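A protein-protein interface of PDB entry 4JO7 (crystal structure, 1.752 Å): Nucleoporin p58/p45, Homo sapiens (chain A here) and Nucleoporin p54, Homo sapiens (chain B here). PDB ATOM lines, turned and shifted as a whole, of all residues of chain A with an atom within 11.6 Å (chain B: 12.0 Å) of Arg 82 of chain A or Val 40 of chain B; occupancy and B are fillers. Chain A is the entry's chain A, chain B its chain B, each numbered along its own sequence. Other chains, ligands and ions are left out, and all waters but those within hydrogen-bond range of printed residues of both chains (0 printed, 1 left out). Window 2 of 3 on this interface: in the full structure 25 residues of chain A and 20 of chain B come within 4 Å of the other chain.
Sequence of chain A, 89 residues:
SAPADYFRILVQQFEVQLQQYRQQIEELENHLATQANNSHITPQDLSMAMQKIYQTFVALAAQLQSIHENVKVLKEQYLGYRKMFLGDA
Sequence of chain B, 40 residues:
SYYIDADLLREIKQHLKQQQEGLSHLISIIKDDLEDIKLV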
ATOM      1  N   LYS A  72      26.206  14.783  19.842  1.00  0.00           N
ATOM      2  CA  LYS A  72      26.080  15.495  21.109  1.00  0.00           C
ATOM      3  C   LYS A  72      26.239  17.000  20.898  1.00  0.00           C
ATOM      4  O   LYS A  72      25.493  17.792  21.468  1.00  0.00           O
ATOM      5  CB  LYS A  72      27.119  15.013  22.122  1.00  0.00           C
ATOM      6  CG  LYS A  72      26.957  13.576  22.584  1.00  0.00           C
ATOM      7  CD  LYS A  72      27.987  13.262  23.664  1.00  0.00           C
ATOM      8  CE  LYS A  72      27.981  11.783  24.046  1.00  0.00           C
ATOM      9  NZ  LYS A  72      29.058  11.472  25.018  1.00  0.00           N
ATOM     10  N   VAL A  73      27.228  17.392  20.102  1.00  0.00           N
ATOM     11  CA  VAL A  73      27.410  18.797  19.740  1.00  0.00           C
ATOM     12  C   VAL A  73      26.155  19.340  19.060  1.00  0.00           C
ATOM     13  O   VAL A  73      25.668  20.424  19.405  1.00  0.00           O
ATOM     14  CB  VAL A  73      28.643  18.995  18.826  1.00  0.00           C
ATOM     15  CG1 VAL A  73      28.685  20.423  18.270  1.00  0.00           C
ATOM     16  CG2 VAL A  73      29.922  18.663  19.577  1.00  0.00           C
ATOM     17  N   LEU A  74      25.613  18.573  18.119  1.00  0.00           N
ATOM     18  CA  LEU A  74      24.409  18.975  17.407  1.00  0.00           C
ATOM     19  C   LEU A  74      23.281  19.278  18.388  1.00  0.00           C
ATOM     20  O   LEU A  74      22.600  20.302  18.261  1.00  0.00           O
ATOM     21  CB  LEU A  74      23.975  17.889  16.421  1.00  0.00           C
ATOM     22  CG  LEU A  74      22.785  18.223  15.523  1.00  0.00           C
ATOM     23  CD1 LEU A  74      23.116  19.420  14.631  1.00  0.00           C
ATOM     24  CD2 LEU A  74      22.362  17.016  14.674  1.00  0.00           C
ATOM     25  N   LYS A  75      23.099  18.400  19.371  1.00  0.00           N
ATOM     26  CA  LYS A  75      22.057  18.592  20.385  1.00  0.00           C
ATOM     27  C   LYS A  75      22.291  19.871  21.174  1.00  0.00           C
ATOM     28  O   LYS A  75      21.352  20.622  21.426  1.00  0.00           O
ATOM     29  CB  LYS A  75      21.973  17.394  21.335  1.00  0.00           C
ATOM     30  CG  LYS A  75      20.840  17.510  22.355  1.00  0.00           C
ATOM     31  CD  LYS A  75      20.738  16.293  23.258  1.00  0.00           C
ATOM     32  CE  LYS A  75      19.535  16.415  24.190  1.00  0.00           C
ATOM     33  NZ  LYS A  75      19.359  15.198  25.033  1.00  0.00           N
ATOM     34  N   GLU A  76      23.542  20.126  21.554  1.00  0.00           N
ATOM     35  CA  GLU A  76      23.884  21.325  22.316  1.00  0.00           C
ATOM     36  C   GLU A  76      23.552  22.583  21.522  1.00  0.00           C
ATOM     37  O   GLU A  76      23.053  23.574  22.067  1.00  0.00           O
ATOM     38  CB  GLU A  76      25.371  21.334  22.674  1.00  0.00           C
ATOM     39  CG  GLU A  76      25.794  20.234  23.619  1.00  0.00           C
ATOM     40  CD  GLU A  76      27.261  20.329  24.000  1.00  0.00           C
ATOM     41  OE1 GLU A  76      28.030  20.991  23.268  1.00  0.00           O
ATOM     42  OE2 GLU A  76      27.644  19.743  25.035  1.00  0.00           O
ATOM     43  N   GLN A  77      23.836  22.537  20.229  1.00  0.00           N
ATOM     44  CA  GLN A  77      23.564  23.658  19.348  1.00  0.00           C
ATOM     45  C   GLN A  77      22.058  23.866  19.160  1.00  0.00           C
ATOM     46  O   GLN A  77      21.594  25.008  19.100  1.00  0.00           O
ATOM     47  CB  GLN A  77      24.280  23.434  18.016  1.00  0.00           C
ATOM     48  CG  GLN A  77      25.796  23.494  18.170  1.00  0.00           C
ATOM     49  CD  GLN A  77      26.522  23.238  16.868  1.00  0.00           C
ATOM     50  OE1 GLN A  77      25.981  22.614  15.962  1.00  0.00           O
ATOM     51  NE2 GLN A  77      27.756  23.718  16.769  1.00  0.00           N
ATOM     52  N   TYR A  78      21.299  22.773  19.074  1.00  0.00           N
ATOM     53  CA  TYR A  78      19.832  22.860  19.040  1.00  0.00           C
ATOM     54  C   TYR A  78      19.328  23.604  20.270  1.00  0.00           C
ATOM     55  O   TYR A  78      18.506  24.517  20.176  1.00  0.00           O
ATOM     56  CB  TYR A  78      19.182  21.477  19.039  1.00  0.00           C
ATOM     57  CG  TYR A  78      18.993  20.808  17.696  1.00  0.00           C
ATOM     58  CD1 TYR A  78      19.820  21.094  16.617  1.00  0.00           C
ATOM     59  CD2 TYR A  78      17.976  19.886  17.514  1.00  0.00           C
ATOM     60  CE1 TYR A  78      19.638  20.478  15.402  1.00  0.00           C
ATOM     61  CE2 TYR A  78      17.786  19.264  16.308  1.00  0.00           C
ATOM     62  CZ  TYR A  78      18.618  19.556  15.251  1.00  0.00           C
ATOM     63  OH  TYR A  78      18.407  18.920  14.050  1.00  0.00           O
ATOM     64  N   LEU A  79      19.811  23.183  21.430  1.00  0.00           N
ATOM     65  CA  LEU A  79      19.390  23.769  22.702  1.00  0.00           C
ATOM     66  C   LEU A  79      19.786  25.233  22.786  1.00  0.00           C
ATOM     67  O   LEU A  79      19.022  26.068  23.279  1.00  0.00           O
ATOM     68  CB  LEU A  79      20.006  23.000  23.866  1.00  0.00           C
ATOM     69  CG  LEU A  79      19.533  21.554  24.023  1.00  0.00           C
ATOM     70  CD1 LEU A  79      20.268  20.871  25.161  1.00  0.00           C
ATOM     71  CD2 LEU A  79      18.046  21.510  24.257  1.00  0.00           C
ATOM     72  N   GLY A  80      20.980  25.547  22.297  1.00  0.00           N
ATOM     73  CA  GLY A  80      21.446  26.922  22.263  1.00  0.00           C
ATOM     74  C   GLY A  80      20.540  27.786  21.406  1.00  0.00           C
ATOM     75  O   GLY A  80      20.192  28.905  21.789  1.00  0.00           O
ATOM     76  N   TYR A  81      20.151  27.261  20.248  1.00  0.00           N
ATOM     77  CA  TYR A  81      19.255  27.972  19.348  1.00  0.00           C
ATOM     78  C   TYR A  81      17.865  28.167  19.956  1.00  0.00           C
ATOM     79  O   TYR A  81      17.279  29.256  19.882  1.00  0.00           O
ATOM     80  CB  TYR A  81      19.127  27.236  18.015  1.00  0.00           C
ATOM     81  CG  TYR A  81      18.229  27.971  17.051  1.00  0.00           C
ATOM     82  CD1 TYR A  81      18.736  28.947  16.209  1.00  0.00           C
ATOM     83  CD2 TYR A  81      16.867  27.707  17.005  1.00  0.00           C
ATOM     84  CE1 TYR A  81      17.912  29.636  15.333  1.00  0.00           C
ATOM     85  CE2 TYR A  81      16.036  28.389  16.143  1.00  0.00           C
ATOM     86  CZ  TYR A  81      16.562  29.352  15.309  1.00  0.00           C
ATOM     87  OH  TYR A  81      15.729  30.028  14.449  1.00  0.00           O
ATOM     88  N   ARG A  82      17.332  27.109  20.546  1.00  0.00           N
ATOM     89  CA  ARG A  82      16.008  27.162  21.150  1.00  0.00           C
ATOM     90  C   ARG A  82      15.980  28.212  22.259  1.00  0.00           C
ATOM     91  O   ARG A  82      15.043  28.990  22.364  1.00  0.00           O
ATOM     92  CB  ARG A  82      15.635  25.789  21.715  1.00  0.00           C
ATOM     93  CG  ARG A  82      14.232  25.715  22.294  1.00  0.00           C
ATOM     94  CD  ARG A  82      14.117  24.601  23.322  1.00  0.00           C
ATOM     95  NE  ARG A  82      14.357  23.277  22.754  1.00  0.00           N
ATOM     96  CZ  ARG A  82      14.410  22.158  23.470  1.00  0.00           C
ATOM     97  NH1 ARG A  82      14.250  22.208  24.788  1.00  0.00           N
ATOM     98  NH2 ARG A  82      14.632  20.991  22.874  1.00  0.00           N
ATOM     99  N   LYS A  83      17.024  28.234  23.075  1.00  0.00           N
ATOM    100  CA  LYS A  83      17.124  29.175  24.180  1.00  0.00           C
ATOM    101  C   LYS A  83      17.107  30.604  23.647  1.00  0.00           C
ATOM    102  O   LYS A  83      16.428  31.485  24.184  1.00  0.00           O
ATOM    103  CB  LYS A  83      18.420  28.919  24.945  1.00  0.00           C
ATOM    104  CG  LYS A  83      18.636  29.770  26.171  1.00  0.00           C
ATOM    105  CD  LYS A  83      19.989  29.447  26.810  1.00  0.00           C
ATOM    106  CE  LYS A  83      19.835  28.884  28.212  1.00  0.00           C
ATOM    107  NZ  LYS A  83      19.266  29.881  29.159  1.00  0.00           N
ATOM    108  N   MET A  84      17.859  30.827  22.577  1.00  0.00           N
ATOM    109  CA  MET A  84      17.950  32.150  21.975  1.00  0.00           C
ATOM    110  C   MET A  84      16.612  32.551  21.367  1.00  0.00           C
ATOM    111  O   MET A  84      16.141  33.681  21.556  1.00  0.00           O
ATOM    112  CB  MET A  84      19.039  32.145  20.912  1.00  0.00           C
ATOM    113  CG  MET A  84      19.434  33.506  20.398  1.00  0.00           C
ATOM    114  SD  MET A  84      20.857  33.347  19.061  1.00  0.00           S
ATOM    115  CE  MET A  84      22.225  32.501  20.136  1.00  0.00           C
ATOM    116  N   PHE A  85      15.996  31.619  20.642  1.00  0.00           N
ATOM    117  CA  PHE A  85      14.706  31.854  20.010  1.00  0.00           C
ATOM    118  C   PHE A  85      13.665  32.274  21.055  1.00  0.00           C
ATOM    119  O   PHE A  85      12.803  33.107  20.782  1.00  0.00           O
ATOM    120  CB  PHE A  85      14.248  30.595  19.268  1.00  0.00           C
ATOM    121  CG  PHE A  85      13.141  30.833  18.276  1.00  0.00           C
ATOM    122  CD1 PHE A  85      11.814  30.879  18.691  1.00  0.00           C
ATOM    123  CD2 PHE A  85      13.424  30.992  16.924  1.00  0.00           C
ATOM    124  CE1 PHE A  85      10.798  31.090  17.782  1.00  0.00           C
ATOM    125  CE2 PHE A  85      12.414  31.206  16.010  1.00  0.00           C
ATOM    126  CZ  PHE A  85      11.092  31.257  16.441  1.00  0.00           C
ATOM    127  N   LEU A  86      13.768  31.706  22.255  1.00  0.00           N
ATOM    128  CA  LEU A  86      12.809  31.980  23.333  1.00  0.00           C
ATOM    129  C   LEU A  86      13.210  33.184  24.189  1.00  0.00           C
ATOM    130  O   LEU A  86      12.559  33.486  25.187  1.00  0.00           O
ATOM    131  CB  LEU A  86      12.623  30.740  24.214  1.00  0.00           C
ATOM    132  CG  LEU A  86      11.966  29.530  23.543  1.00  0.00           C
ATOM    133  CD1 LEU A  86      11.833  28.378  24.528  1.00  0.00           C
ATOM    134  CD2 LEU A  86      10.614  29.881  22.940  1.00  0.00           C
ATOM    135  N   GLY A  87      14.276  33.870  23.794  1.00  0.00           N
ATOM    136  CA  GLY A  87      14.628  35.153  24.374  1.00  0.00           C
ATOM    137  C   GLY A  87      15.554  35.085  25.572  1.00  0.00           C
ATOM    138  O   GLY A  87      15.642  36.039  26.341  1.00  0.00           O
ATOM    139  N   ASP A  88      16.258  33.971  25.731  1.00  0.00           N
ATOM    140  CA  ASP A  88      17.132  33.798  26.885  1.00  0.00           C
ATOM    141  C   ASP A  88      18.595  33.691  26.475  1.00  0.00           C
ATOM    142  O   ASP A  88      18.930  33.006  25.511  1.00  0.00           O
ATOM    143  CB  ASP A  88      16.721  32.559  27.673  1.00  0.00           C
ATOM    144  CG  ASP A  88      17.364  32.507  29.045  1.00  0.00           C
ATOM    145  OD1 ASP A  88      18.574  32.802  29.149  1.00  0.00           O
ATOM    146  OD2 ASP A  88      16.659  32.181  30.022  1.00  0.00           O
ATOM    147  N   ASP B  33      19.904   8.292  19.238  1.00  0.00           N
ATOM    148  CA  ASP B  33      20.224   9.698  19.476  1.00  0.00           C
ATOM    149  C   ASP B  33      19.586  10.606  18.424  1.00  0.00           C
ATOM    150  O   ASP B  33      18.961  11.611  18.758  1.00  0.00           O
ATOM    151  CB  ASP B  33      21.738   9.917  19.486  1.00  0.00           C
ATOM    152  CG  ASP B  33      22.424   9.238  20.653  1.00  0.00           C
ATOM    153  OD1 ASP B  33      21.759   8.969  21.671  1.00  0.00           O
ATOM    154  OD2 ASP B  33      23.643   8.983  20.559  1.00  0.00           O
ATOM    155  N   LEU B  34      19.738  10.251  17.152  1.00  0.00           N
ATOM    156  CA  LEU B  34      19.207  11.078  16.063  1.00  0.00           C
ATOM    157  C   LEU B  34      17.679  11.140  16.049  1.00  0.00           C
ATOM    158  O   LEU B  34      17.088  12.129  15.605  1.00  0.00           O
ATOM    159  CB  LEU B  34      19.710  10.568  14.711  1.00  0.00           C
ATOM    160  CG  LEU B  34      21.189  10.826  14.419  1.00  0.00           C
ATOM    161  CD1 LEU B  34      21.613  10.101  13.168  1.00  0.00           C
ATOM    162  CD2 LEU B  34      21.462  12.320  14.291  1.00  0.00           C
ATOM    163  N   GLU B  35      17.039  10.081  16.516  1.00  0.00           N
ATOM    164  CA  GLU B  35      15.589  10.042  16.561  1.00  0.00           C
ATOM    165  C   GLU B  35      15.068  10.913  17.702  1.00  0.00           C
ATOM    166  O   GLU B  35      13.985  11.485  17.613  1.00  0.00           O
ATOM    167  CB  GLU B  35      15.100   8.599  16.728  1.00  0.00           C
ATOM    168  CG  GLU B  35      13.621   8.474  17.070  1.00  0.00           C
ATOM    169  CD  GLU B  35      12.724   9.075  16.005  1.00  0.00           C
ATOM    170  OE1 GLU B  35      13.088   9.000  14.812  1.00  0.00           O
ATOM    171  OE2 GLU B  35      11.660   9.629  16.359  1.00  0.00           O
ATOM    172  N   ASP B  36      15.856  11.020  18.765  1.00  0.00           N
ATOM    173  CA  ASP B  36      15.399  11.646  20.002  1.00  0.00           C
ATOM    174  C   ASP B  36      15.631  13.160  20.062  1.00  0.00           C
ATOM    175  O   ASP B  36      14.875  13.874  20.724  1.00  0.00           O
ATOM    176  CB  ASP B  36      16.070  10.981  21.205  1.00  0.00           C
ATOM    177  CG  ASP B  36      15.556  11.518  22.521  1.00  0.00           C
ATOM    178  OD1 ASP B  36      14.368  11.298  22.821  1.00  0.00           O
ATOM    179  OD2 ASP B  36      16.337  12.161  23.253  1.00  0.00           O
ATOM    180  N   ILE B  37      16.677  13.635  19.391  1.00  0.00           N
ATOM    181  CA  ILE B  37      17.001  15.064  19.344  1.00  0.00           C
ATOM    182  C   ILE B  37      15.850  15.878  18.745  1.00  0.00           C
ATOM    183  O   ILE B  37      15.314  15.537  17.685  1.00  0.00           O
ATOM    184  CB  ILE B  37      18.288  15.327  18.514  1.00  0.00           C
ATOM    185  CG1 ILE B  37      19.512  14.698  19.183  1.00  0.00           C
ATOM    186  CG2 ILE B  37      18.515  16.808  18.320  1.00  0.00           C
ATOM    187  CD1 ILE B  37      19.402  14.575  20.670  1.00  0.00           C
ATOM    188  N   LYS B  38      15.487  16.957  19.436  1.00  0.00           N
ATOM    189  CA  LYS B  38      14.356  17.804  19.066  1.00  0.00           C
ATOM    190  C   LYS B  38      14.767  19.266  19.142  1.00  0.00           C
ATOM    191  O   LYS B  38      15.311  19.692  20.156  1.00  0.00           O
ATOM    192  CB  LYS B  38      13.206  17.614  20.066  1.00  0.00           C
ATOM    193  CG  LYS B  38      12.608  16.232  20.130  1.00  0.00           C
ATOM    194  CD  LYS B  38      11.622  16.134  21.289  1.00  0.00           C
ATOM    195  CE  LYS B  38      11.099  14.722  21.473  1.00  0.00           C
ATOM    196  NZ  LYS B  38      12.185  13.760  21.829  1.00  0.00           N
ATOM    197  N   LEU B  39      14.505  20.042  18.094  1.00  0.00           N
ATOM    198  CA  LEU B  39      14.800  21.473  18.162  1.00  0.00           C
ATOM    199  C   LEU B  39      13.976  22.082  19.285  1.00  0.00           C
ATOM    200  O   LEU B  39      14.448  22.959  20.009  1.00  0.00           O
ATOM    201  CB  LEU B  39      14.497  22.176  16.839  1.00  0.00           C
ATOM    202  CG  LEU B  39      14.905  23.655  16.815  1.00  0.00           C
ATOM    203  CD1 LEU B  39      16.403  23.802  17.003  1.00  0.00           C
ATOM    204  CD2 LEU B  39      14.466  24.341  15.523  1.00  0.00           C
ATOM    205  N   VAL B  40      12.745  21.592  19.425  1.00  0.00           N
ATOM    206  CA  VAL B  40      11.861  21.963  20.524  1.00  0.00           C
ATOM    207  C   VAL B  40      10.763  20.910  20.657  1.00  0.00           C
ATOM    208  O   VAL B  40      10.563  20.094  19.747  1.00  0.00           O
ATOM    209  CB  VAL B  40      11.221  23.349  20.296  1.00  0.00           C
ATOM    210  CG1 VAL B  40      10.208  23.295  19.158  1.00  0.00           C
ATOM    211  CG2 VAL B  40      10.566  23.845  21.575  1.00  0.00           C
ATOM    212  OXT VAL B  40      10.052  20.835  21.661  1.00  0.00           O
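The backbone carbonyl oxygen (O) of Lys 38 of chain B sits at hydrogen-bond distance from the guanidinium group (NH2) of Arg 82 of chain A (3.1 Å).
O of Leu 39 of chain B sits at hydrogen-bond distance from NE of Arg 82 of chain A (2.8 Å).
The side-chain amino group (NZ) of Lys 38 of chain B lies within salt-bridge range of the side-chain carboxylate (OD1) of Asp 36 of chain B.
Lys 75 of chain A touches Ile 37 of chain B.
Tyr 78 of chain A touches Ile 37 of chain B (CD2 to CG2, 3.2 Å).
C of Lys 38 of chain B touches CD2 of Tyr 78 of chain A, 3.7 Å away.
Tyr 78 of chain A touches Leu 39 of chain B (CD2 to N, 3.5 Å).
Tyr 81 of chain A touches Leu 39 of chain B.
Arg 82 of chain A touches Val 40 of chain B (NE to CA, 3.6 Å).
Of the printed residues of chain B, Lys 75 of chain A touches Ile 37 (3.4 Å).
Printed residues of chain B within 4 Å of Tyr 78 of chain A: Ile 37 (3.2 Å), Lys 38 (3.7 Å) and Leu 39 (3.5 Å).
No residue of chain B comes within 4 Å of Gly 80 of chain A.
Tyr 81 of chain A touches just one residue of chain B: Leu 39.
No residue of chain B comes within 4 Å of Lys 83 of chain A.
No residue of chain B comes within 4 Å of Phe 85 of chain A.
No residue of chain B comes within 4 Å of Leu 86 of chain A.
Gly 87 of chain A touches none of the printed residues of chain B.
Of the printed residues of chain A, Ile 37 of chain B touches Lys 75 (3.4 Å) and Tyr 78 (3.2 Å).
Lys 38 of chain B touches two residues of chain A.
Leu 39 of chain B touches just these residues of chain A: Tyr 78, Tyr 81 and Arg 82.
Of chain A, only Arg 82 comes within 4 Å of Val 40 of chain B.
The nearest residue of chain B that does not touch Arg 82 of chain A is Ile 37 of chain B (6.7 Å).
The nearest residue of chain A that does not touch Val 40 of chain B is Leu 86 of chain A (5.6 Å).
Hydrophobic or aromatic side chains of chain B that line the printed part of chain A: Ile 37, Leu 39 and Val 40.
Printed residues of chain A that touch a printed residue of chain B: Lys 75, Tyr 78, Tyr 81 and Arg 82.
Hydrophobic or aromatic side chains of chain A that line the printed part of chain B: Tyr 78 and Tyr 81.
Among the printed residues, 8 pairs touch across the chains.
Among the printed residues, no Asp or Glu carboxylate lies within 4 Å of a Lys or Arg side-chain nitrogen of the other chain.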
